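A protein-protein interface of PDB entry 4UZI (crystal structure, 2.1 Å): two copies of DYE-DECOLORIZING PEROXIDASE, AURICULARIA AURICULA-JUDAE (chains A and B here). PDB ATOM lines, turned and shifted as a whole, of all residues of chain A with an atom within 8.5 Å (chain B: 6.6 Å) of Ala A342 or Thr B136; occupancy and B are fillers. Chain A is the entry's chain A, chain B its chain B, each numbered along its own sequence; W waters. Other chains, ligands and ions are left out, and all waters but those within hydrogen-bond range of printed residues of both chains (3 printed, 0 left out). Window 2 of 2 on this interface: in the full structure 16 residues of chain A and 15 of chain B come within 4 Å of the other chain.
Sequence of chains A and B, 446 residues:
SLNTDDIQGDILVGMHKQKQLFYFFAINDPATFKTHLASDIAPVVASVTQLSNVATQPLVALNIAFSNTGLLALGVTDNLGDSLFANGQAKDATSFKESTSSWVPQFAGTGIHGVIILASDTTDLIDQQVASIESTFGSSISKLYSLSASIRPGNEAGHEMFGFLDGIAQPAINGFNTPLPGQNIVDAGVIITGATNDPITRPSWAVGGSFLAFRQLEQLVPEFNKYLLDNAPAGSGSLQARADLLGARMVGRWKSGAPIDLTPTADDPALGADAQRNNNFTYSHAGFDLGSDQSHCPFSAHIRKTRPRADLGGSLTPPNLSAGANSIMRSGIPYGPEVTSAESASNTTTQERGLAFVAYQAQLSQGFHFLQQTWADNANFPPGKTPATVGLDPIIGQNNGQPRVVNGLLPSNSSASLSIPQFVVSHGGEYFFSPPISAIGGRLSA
OG of Ser B135 lies within hydrogen-bond range of OG1 of Thr A340, 2.7 Å away. NE2 of Gln A351 lies within hydrogen-bond range of OE1 of Glu B134, at 3.0 Å.
The side-chain hydroxyl (OG1) of Thr B136 lies within hydrogen-bond range of the backbone carbonyl oxygen (O) of Ser B132, 2.6 Å away. The side-chain carboxylate of Glu A343 lies within hydrogen-bond range of the side-chain hydroxyl of Thr A340, at 2.7 Å. O of Glu A343 is in hydrogen-bond range of OG of Ser A346, at 3.1 Å. O of Glu A343 is in hydrogen-bond range of N of Thr A348 (3.1 Å). The backbone NH (N) of Thr A350 is in hydrogen-bond range of the side-chain carboxylate (OE2) of Glu A343 (3.0 Å). The side-chain carboxylate (OE1) of Glu A343 lies within salt-bridge range of the guanidinium group (NH2) of Arg A353 (2.6 Å).
Among the printed residues, merely in contact across the chains: Thr A350 with Ser B135 (3.1 Å), Ala A342 with Ser B135 (3.3 Å), Gln A351 with Ala B131 (3.5 Å), Thr A340 with Ser B132 (3.6 Å), Gln A351 with Ser B135 (3.6 Å), Glu A343 with Ser B135 (3.7 Å), Ala A342 with Thr B136 (3.7 Å) and Thr A340 with Ala B131 (3.8 Å).
Ala A342 touches just these residues of chain B: Ser B135 and Thr B136. Thr B136 touches one residue of chain A. Ser B135 touches five residues of chain A. Printed residues of chain A within 4 Å of Glu B134: Gln A351. Of the printed residues of chain B, Thr A350 touches Ser B135 (3.1 Å). Of the printed residues of chain B, Gln A351 touches Ala B131, Glu B134 and Ser B135. Printed residues of chain A within 4 Å of Ser B132: Thr A340 (3.6 Å). Of the printed residues of chain B, Glu A343 touches Ser B135. Arg A353 touches none of the printed residues of chain B. Thr B32 touches none of the printed residues of chain A. The nearest residue of chain B that does not touch Ala A342 is Ser B132 (5.0 Å). The nearest printed residue of chain A that does not touch Thr B136 is Ser A341 (5.7 Å).
Hydrophobic or aromatic side chains of chain A that line the printed part of chain B: Ala A342. Of the 14 printed residues of chain B, 5 touch a printed residue of chain A. Among the printed residues, 10 pairs touch across the chains. Among the printed residues, no Asp or Glu carboxylate lies within 4 Å of a Lys or Arg side-chain nitrogen of the other chain.
No position is printed for both chains. Of the 10 pairs that touch across the chains among the printed residues, none has its exchanged pair printed and touching as well.
Water W1 bridges OG of Ser A341 (2.6 Å) and OG of Ser B132 (3.1 Å). Water W2 lies within hydrogen-bond range of OG of Ser B135 (3.0 Å), N of Ala A342 (3.0 Å), O of Ser B132 (3.1 Å) and OG1 of Thr B136 (3.2 Å). Water W3 bridges O of Ser B135 and OG of Ser A346.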
ATOM      1  N   PRO A 222      -3.001  14.108 -30.875  1.00  0.00           N
ATOM      2  CA  PRO A 222      -4.366  14.593 -30.696  1.00  0.00           C
ATOM      3  C   PRO A 222      -4.632  15.822 -31.554  1.00  0.00           C
ATOM      4  O   PRO A 222      -5.683  15.920 -32.188  1.00  0.00           O
ATOM      5  CB  PRO A 222      -4.414  14.959 -29.211  1.00  0.00           C
ATOM      6  CG  PRO A 222      -3.343  14.126 -28.579  1.00  0.00           C
ATOM      7  CD  PRO A 222      -2.250  14.091 -29.606  1.00  0.00           C
ATOM      8  N   VAL A 339      -1.087   7.687 -26.875  1.00  0.00           N
ATOM      9  CA  VAL A 339      -2.055   8.733 -26.564  1.00  0.00           C
ATOM     10  C   VAL A 339      -2.997   8.303 -25.440  1.00  0.00           C
ATOM     11  O   VAL A 339      -3.573   7.215 -25.479  1.00  0.00           O
ATOM     12  CB  VAL A 339      -2.898   9.096 -27.808  1.00  0.00           C
ATOM     13  CG1 VAL A 339      -3.969  10.113 -27.448  1.00  0.00           C
ATOM     14  CG2 VAL A 339      -2.002   9.625 -28.921  1.00  0.00           C
ATOM     15  N   THR A 340      -3.160   9.149 -24.432  1.00  0.00           N
ATOM     16  CA  THR A 340      -4.053   8.811 -23.315  1.00  0.00           C
ATOM     17  C   THR A 340      -5.478   9.293 -23.549  1.00  0.00           C
ATOM     18  O   THR A 340      -5.726  10.084 -24.460  1.00  0.00           O
ATOM     19  CB  THR A 340      -3.530   9.374 -21.986  1.00  0.00           C
ATOM     20  OG1 THR A 340      -3.432  10.802 -22.076  1.00  0.00           O
ATOM     21  CG2 THR A 340      -2.152   8.800 -21.683  1.00  0.00           C
ATOM     22  N   SER A 341      -6.420   8.791 -22.747  1.00  0.00           N
ATOM     23  CA  SER A 341      -7.820   9.198 -22.871  1.00  0.00           C
ATOM     24  C   SER A 341      -8.018  10.684 -22.586  1.00  0.00           C
ATOM     25  O   SER A 341      -8.798  11.352 -23.266  1.00  0.00           O
ATOM     26  CB  SER A 341      -8.735   8.354 -21.975  1.00  0.00           C
ATOM     27  OG  SER A 341      -8.069   7.937 -20.794  1.00  0.00           O
ATOM     28  N   ALA A 342      -7.329  11.193 -21.571  1.00  0.00           N
ATOM     29  CA  ALA A 342      -7.382  12.620 -21.257  1.00  0.00           C
ATOM     30  C   ALA A 342      -6.931  13.493 -22.427  1.00  0.00           C
ATOM     31  O   ALA A 342      -7.634  14.422 -22.820  1.00  0.00           O
ATOM     32  CB  ALA A 342      -6.564  12.930 -20.015  1.00  0.00           C
ATOM     33  N   GLU A 343      -5.786  13.159 -23.017  1.00  0.00           N
ATOM     34  CA  GLU A 343      -5.276  13.921 -24.154  1.00  0.00           C
ATOM     35  C   GLU A 343      -6.217  13.811 -25.345  1.00  0.00           C
ATOM     36  O   GLU A 343      -6.464  14.786 -26.046  1.00  0.00           O
ATOM     37  CB  GLU A 343      -3.880  13.441 -24.542  1.00  0.00           C
ATOM     38  CG  GLU A 343      -2.857  13.526 -23.415  1.00  0.00           C
ATOM     39  CD  GLU A 343      -1.544  12.854 -23.775  1.00  0.00           C
ATOM     40  OE1 GLU A 343      -1.496  11.606 -23.790  1.00  0.00           O
ATOM     41  OE2 GLU A 343      -0.574  13.572 -24.099  1.00  0.00           O
ATOM     42  N   SER A 344      -6.722  12.605 -25.584  1.00  0.00           N
ATOM     43  CA  SER A 344      -7.601  12.374 -26.711  1.00  0.00           C
ATOM     44  C   SER A 344      -8.903  13.148 -26.528  1.00  0.00           C
ATOM     45  O   SER A 344      -9.328  13.884 -27.415  1.00  0.00           O
ATOM     46  CB  SER A 344      -7.889  10.881 -26.864  1.00  0.00           C
ATOM     47  OG  SER A 344      -8.720  10.659 -27.987  1.00  0.00           O
ATOM     48  N   ALA A 345      -9.500  13.020 -25.350  1.00  0.00           N
ATOM     49  CA  ALA A 345     -10.718  13.754 -25.016  1.00  0.00           C
ATOM     50  C   ALA A 345     -10.553  15.260 -25.194  1.00  0.00           C
ATOM     51  O   ALA A 345     -11.470  15.939 -25.650  1.00  0.00           O
ATOM     52  CB  ALA A 345     -11.152  13.434 -23.593  1.00  0.00           C
ATOM     53  N   SER A 346      -9.377  15.774 -24.850  1.00  0.00           N
ATOM     54  CA  SER A 346      -9.127  17.216 -24.851  1.00  0.00           C
ATOM     55  C   SER A 346      -8.561  17.728 -26.169  1.00  0.00           C
ATOM     56  O   SER A 346      -8.454  18.938 -26.372  1.00  0.00           O
ATOM     57  CB  SER A 346      -8.155  17.578 -23.725  1.00  0.00           C
ATOM     58  OG  SER A 346      -6.913  16.914 -23.903  1.00  0.00           O
ATOM     59  N   ASN A 347      -8.107  16.815 -27.021  1.00  0.00           N
ATOM     60  CA  ASN A 347      -7.434  17.201 -28.251  1.00  0.00           C
ATOM     61  C   ASN A 347      -6.101  17.890 -28.005  1.00  0.00           C
ATOM     62  O   ASN A 347      -5.669  18.696 -28.817  1.00  0.00           O
ATOM     63  CB  ASN A 347      -8.324  18.133 -29.083  1.00  0.00           C
ATOM     64  CG  ASN A 347      -9.631  17.487 -29.489  1.00  0.00           C
ATOM     65  OD1 ASN A 347      -9.674  16.309 -29.840  1.00  0.00           O
ATOM     66  ND2 ASN A 347     -10.709  18.260 -29.443  1.00  0.00           N
ATOM     67  N   THR A 348      -5.443  17.558 -26.901  1.00  0.00           N
ATOM     68  CA  THR A 348      -4.291  18.327 -26.449  1.00  0.00           C
ATOM     69  C   THR A 348      -3.204  17.424 -25.878  1.00  0.00           C
ATOM     70  O   THR A 348      -3.447  16.635 -24.966  1.00  0.00           O
ATOM     71  CB  THR A 348      -4.696  19.368 -25.381  1.00  0.00           C
ATOM     72  OG1 THR A 348      -5.674  20.263 -25.927  1.00  0.00           O
ATOM     73  CG2 THR A 348      -3.484  20.175 -24.927  1.00  0.00           C
ATOM     74  N   THR A 349      -1.995  17.563 -26.405  1.00  0.00           N
ATOM     75  CA  THR A 349      -0.851  16.816 -25.902  1.00  0.00           C
ATOM     76  C   THR A 349      -0.382  17.361 -24.562  1.00  0.00           C
ATOM     77  O   THR A 349      -0.222  18.576 -24.403  1.00  0.00           O
ATOM     78  CB  THR A 349       0.320  16.881 -26.898  1.00  0.00           C
ATOM     79  OG1 THR A 349      -0.104  16.340 -28.154  1.00  0.00           O
ATOM     80  CG2 THR A 349       1.526  16.092 -26.373  1.00  0.00           C
ATOM     81  N   THR A 350      -0.136  16.459 -23.613  1.00  0.00           N
ATOM     82  CA  THR A 350       0.573  16.798 -22.378  1.00  0.00           C
ATOM     83  C   THR A 350       1.766  15.888 -22.140  1.00  0.00           C
ATOM     84  O   THR A 350       2.633  16.198 -21.324  1.00  0.00           O
ATOM     85  CB  THR A 350      -0.342  16.664 -21.143  1.00  0.00           C
ATOM     86  OG1 THR A 350      -0.718  15.288 -20.976  1.00  0.00           O
ATOM     87  CG2 THR A 350      -1.585  17.510 -21.308  1.00  0.00           C
ATOM     88  N   GLN A 351       1.762  14.720 -22.773  1.00  0.00           N
ATOM     89  CA  GLN A 351       2.866  13.776 -22.631  1.00  0.00           C
ATOM     90  C   GLN A 351       3.675  13.748 -23.923  1.00  0.00           C
ATOM     91  O   GLN A 351       3.115  13.555 -25.002  1.00  0.00           O
ATOM     92  CB  GLN A 351       2.340  12.367 -22.325  1.00  0.00           C
ATOM     93  CG  GLN A 351       1.191  12.315 -21.323  1.00  0.00           C
ATOM     94  CD  GLN A 351       1.564  12.886 -19.967  1.00  0.00           C
ATOM     95  OE1 GLN A 351       1.081  13.949 -19.574  1.00  0.00           O
ATOM     96  NE2 GLN A 351       2.460  12.201 -19.258  1.00  0.00           N
ATOM     97  N   ARG A 353       5.490  12.554 -26.936  1.00  0.00           N
ATOM     98  CA  ARG A 353       5.699  11.359 -27.738  1.00  0.00           C
ATOM     99  C   ARG A 353       6.167  11.819 -29.104  1.00  0.00           C
ATOM    100  O   ARG A 353       6.066  13.009 -29.424  1.00  0.00           O
ATOM    101  CB  ARG A 353       4.401  10.553 -27.855  1.00  0.00           C
ATOM    102  CG  ARG A 353       3.240  11.340 -28.446  1.00  0.00           C
ATOM    103  CD  ARG A 353       1.939  10.552 -28.413  1.00  0.00           C
ATOM    104  NE  ARG A 353       1.548  10.206 -27.044  1.00  0.00           N
ATOM    105  CZ  ARG A 353       0.934  11.040 -26.206  1.00  0.00           C
ATOM    106  NH1 ARG A 353       0.612  12.264 -26.600  1.00  0.00           N
ATOM    107  NH2 ARG A 353       0.637  10.645 -24.970  1.00  0.00           N
ATOM    108  N   THR B  32      -9.007  21.144  -8.430  1.00  0.00           N
ATOM    109  CA  THR B  32      -8.851  20.277  -9.598  1.00  0.00           C
ATOM    110  C   THR B  32      -8.390  18.886  -9.183  1.00  0.00           C
ATOM    111  O   THR B  32      -8.916  17.876  -9.653  1.00  0.00           O
ATOM    112  CB  THR B  32      -7.842  20.862 -10.598  1.00  0.00           C
ATOM    113  OG1 THR B  32      -8.313  22.127 -11.067  1.00  0.00           O
ATOM    114  CG2 THR B  32      -7.658  19.928 -11.777  1.00  0.00           C
ATOM    115  N   HIS B  36     -10.329  14.890  -9.880  1.00  0.00           N
ATOM    116  CA  HIS B  36      -9.722  13.733 -10.505  1.00  0.00           C
ATOM    117  C   HIS B  36      -9.418  12.648  -9.485  1.00  0.00           C
ATOM    118  O   HIS B  36      -9.516  11.462  -9.796  1.00  0.00           O
ATOM    119  CB  HIS B  36      -8.472  14.131 -11.293  1.00  0.00           C
ATOM    120  CG  HIS B  36      -8.756  15.070 -12.423  1.00  0.00           C
ATOM    121  ND1 HIS B  36      -9.615  14.754 -13.453  1.00  0.00           N
ATOM    122  CD2 HIS B  36      -8.331  16.333 -12.663  1.00  0.00           C
ATOM    123  CE1 HIS B  36      -9.696  15.776 -14.285  1.00  0.00           C
ATOM    124  NE2 HIS B  36      -8.925  16.746 -13.829  1.00  0.00           N
ATOM    125  N   ASP B  40     -11.319   9.634 -10.970  1.00  0.00           N
ATOM    126  CA  ASP B  40     -10.385   8.890 -11.802  1.00  0.00           C
ATOM    127  C   ASP B  40      -9.514   7.926 -11.009  1.00  0.00           C
ATOM    128  O   ASP B  40      -9.259   6.802 -11.450  1.00  0.00           O
ATOM    129  CB  ASP B  40      -9.533   9.848 -12.629  1.00  0.00           C
ATOM    130  CG  ASP B  40     -10.350  10.594 -13.660  1.00  0.00           C
ATOM    131  OD1 ASP B  40     -10.958   9.926 -14.524  1.00  0.00           O
ATOM    132  OD2 ASP B  40     -10.437  11.838 -13.569  1.00  0.00           O
ATOM    133  N   ILE B  41      -9.091   8.338  -9.821  1.00  0.00           N
ATOM    134  CA  ILE B  41      -8.277   7.462  -8.989  1.00  0.00           C
ATOM    135  C   ILE B  41      -9.133   6.523  -8.152  1.00  0.00           C
ATOM    136  O   ILE B  41      -8.990   5.303  -8.227  1.00  0.00           O
ATOM    137  CB  ILE B  41      -7.326   8.258  -8.085  1.00  0.00           C
ATOM    138  CG1 ILE B  41      -6.417   9.138  -8.943  1.00  0.00           C
ATOM    139  CG2 ILE B  41      -6.502   7.315  -7.220  1.00  0.00           C
ATOM    140  CD1 ILE B  41      -5.240   8.401  -9.539  1.00  0.00           C
ATOM    141  N   ALA B 131       1.664   8.075 -17.700  1.00  0.00           N
ATOM    142  CA  ALA B 131       1.198   9.010 -18.716  1.00  0.00           C
ATOM    143  C   ALA B 131      -0.265   9.361 -18.467  1.00  0.00           C
ATOM    144  O   ALA B 131      -0.629  10.530 -18.416  1.00  0.00           O
ATOM    145  CB  ALA B 131       1.379   8.433 -20.113  1.00  0.00           C
ATOM    146  N   SER B 132      -1.085   8.334 -18.275  1.00  0.00           N
ATOM    147  CA  SER B 132      -2.523   8.504 -18.107  1.00  0.00           C
ATOM    148  C   SER B 132      -2.868   9.349 -16.877  1.00  0.00           C
ATOM    149  O   SER B 132      -3.749  10.205 -16.933  1.00  0.00           O
ATOM    150  CB  SER B 132      -3.202   7.136 -18.016  1.00  0.00           C
ATOM    151  OG  SER B 132      -4.608   7.265 -18.003  1.00  0.00           O
ATOM    152  N   ILE B 133      -2.162   9.109 -15.777  1.00  0.00           N
ATOM    153  CA  ILE B 133      -2.359   9.868 -14.551  1.00  0.00           C
ATOM    154  C   ILE B 133      -1.958  11.334 -14.714  1.00  0.00           C
ATOM    155  O   ILE B 133      -2.620  12.226 -14.188  1.00  0.00           O
ATOM    156  CB  ILE B 133      -1.541   9.277 -13.385  1.00  0.00           C
ATOM    157  CG1 ILE B 133      -2.099   7.920 -12.956  1.00  0.00           C
ATOM    158  CG2 ILE B 133      -1.505  10.251 -12.214  1.00  0.00           C
ATOM    159  CD1 ILE B 133      -1.179   7.170 -12.010  1.00  0.00           C
ATOM    160  N   GLU B 134      -0.847  11.572 -15.401  1.00  0.00           N
ATOM    161  CA  GLU B 134      -0.320  12.922 -15.540  1.00  0.00           C
ATOM    162  C   GLU B 134      -1.207  13.783 -16.431  1.00  0.00           C
ATOM    163  O   GLU B 134      -1.391  14.968 -16.171  1.00  0.00           O
ATOM    164  CB  GLU B 134       1.119  12.894 -16.064  1.00  0.00           C
ATOM    165  CG  GLU B 134       2.119  12.339 -15.054  1.00  0.00           C
ATOM    166  CD  GLU B 134       3.564  12.453 -15.513  1.00  0.00           C
ATOM    167  OE1 GLU B 134       3.799  12.823 -16.681  1.00  0.00           O
ATOM    168  OE2 GLU B 134       4.470  12.171 -14.698  1.00  0.00           O
ATOM    169  N   SER B 135      -1.759  13.187 -17.480  1.00  0.00           N
ATOM    170  CA  SER B 135      -2.596  13.934 -18.410  1.00  0.00           C
ATOM    171  C   SER B 135      -3.985  14.141 -17.823  1.00  0.00           C
ATOM    172  O   SER B 135      -4.669  15.103 -18.160  1.00  0.00           O
ATOM    173  CB  SER B 135      -2.698  13.202 -19.748  1.00  0.00           C
ATOM    174  OG  SER B 135      -3.425  11.996 -19.602  1.00  0.00           O
ATOM    175  N   THR B 136      -4.410  13.214 -16.972  1.00  0.00           N
ATOM    176  CA  THR B 136      -5.677  13.343 -16.266  1.00  0.00           C
ATOM    177  C   THR B 136      -5.625  14.544 -15.322  1.00  0.00           C
ATOM    178  O   THR B 136      -6.478  15.426 -15.373  1.00  0.00           O
ATOM    179  CB  THR B 136      -5.979  12.071 -15.442  1.00  0.00           C
ATOM    180  OG1 THR B 136      -6.201  10.968 -16.324  1.00  0.00           O
ATOM    181  CG2 THR B 136      -7.198  12.270 -14.552  1.00  0.00           C
ATOM    182  N   PHE B 137      -4.599  14.566 -14.476  1.00  0.00           N
ATOM    183  CA  PHE B 137      -4.420  15.614 -13.483  1.00  0.00           C
ATOM    184  C   PHE B 137      -3.896  16.919 -14.079  1.00  0.00           C
ATOM    185  O   PHE B 137      -4.102  17.994 -13.512  1.00  0.00           O
ATOM    186  CB  PHE B 137      -3.484  15.120 -12.369  1.00  0.00           C
ATOM    187  CG  PHE B 137      -4.182  14.298 -11.323  1.00  0.00           C
ATOM    188  CD1 PHE B 137      -4.464  12.967 -11.552  1.00  0.00           C
ATOM    189  CD2 PHE B 137      -4.664  14.891 -10.168  1.00  0.00           C
ATOM    190  CE1 PHE B 137      -5.173  12.222 -10.626  1.00  0.00           C
ATOM    191  CE2 PHE B 137      -5.371  14.156  -9.239  1.00  0.00           C
ATOM    192  CZ  PHE B 137      -5.627  12.818  -9.465  1.00  0.00           C
ATOM    193  N   GLY B 138      -3.170  16.818 -15.191  1.00  0.00           N
ATOM    194  CA  GLY B 138      -2.560  17.991 -15.806  1.00  0.00           C
ATOM    195  C   GLY B 138      -1.719  18.793 -14.827  1.00  0.00           C
ATOM    196  O   GLY B 138      -0.907  18.242 -14.076  1.00  0.00           O
ATOM    197  N   SER B 139      -1.952  20.096 -14.796  1.00  0.00           N
ATOM    198  CA  SER B 139      -1.149  20.989 -13.980  1.00  0.00           C
ATOM    199  C   SER B 139      -1.491  20.930 -12.487  1.00  0.00           C
ATOM    200  O   SER B 139      -0.869  21.626 -11.687  1.00  0.00           O
ATOM    201  CB  SER B 139      -1.304  22.423 -14.476  1.00  0.00           C
ATOM    202  OG  SER B 139      -2.665  22.822 -14.404  1.00  0.00           O
ATOM    203  N   SER B 140      -2.479  20.123 -12.109  1.00  0.00           N
ATOM    204  CA  SER B 140      -2.882  20.059 -10.705  1.00  0.00           C
ATOM    205  C   SER B 140      -1.882  19.285  -9.842  1.00  0.00           C
ATOM    206  O   SER B 140      -1.926  19.349  -8.615  1.00  0.00           O
ATOM    207  CB  SER B 140      -4.298  19.495 -10.546  1.00  0.00           C
ATOM    208  OG  SER B 140      -4.377  18.139 -10.957  1.00  0.00           O
HETATM  209  O   HOH W   1      -5.711   6.868 -20.821  1.00  0.00           O
HETATM  210  O   HOH W   2      -5.687  10.025 -19.307  1.00  0.00           O
HETATM  211  O   HOH W   3      -4.880  16.234 -21.283  1.00  0.00           O
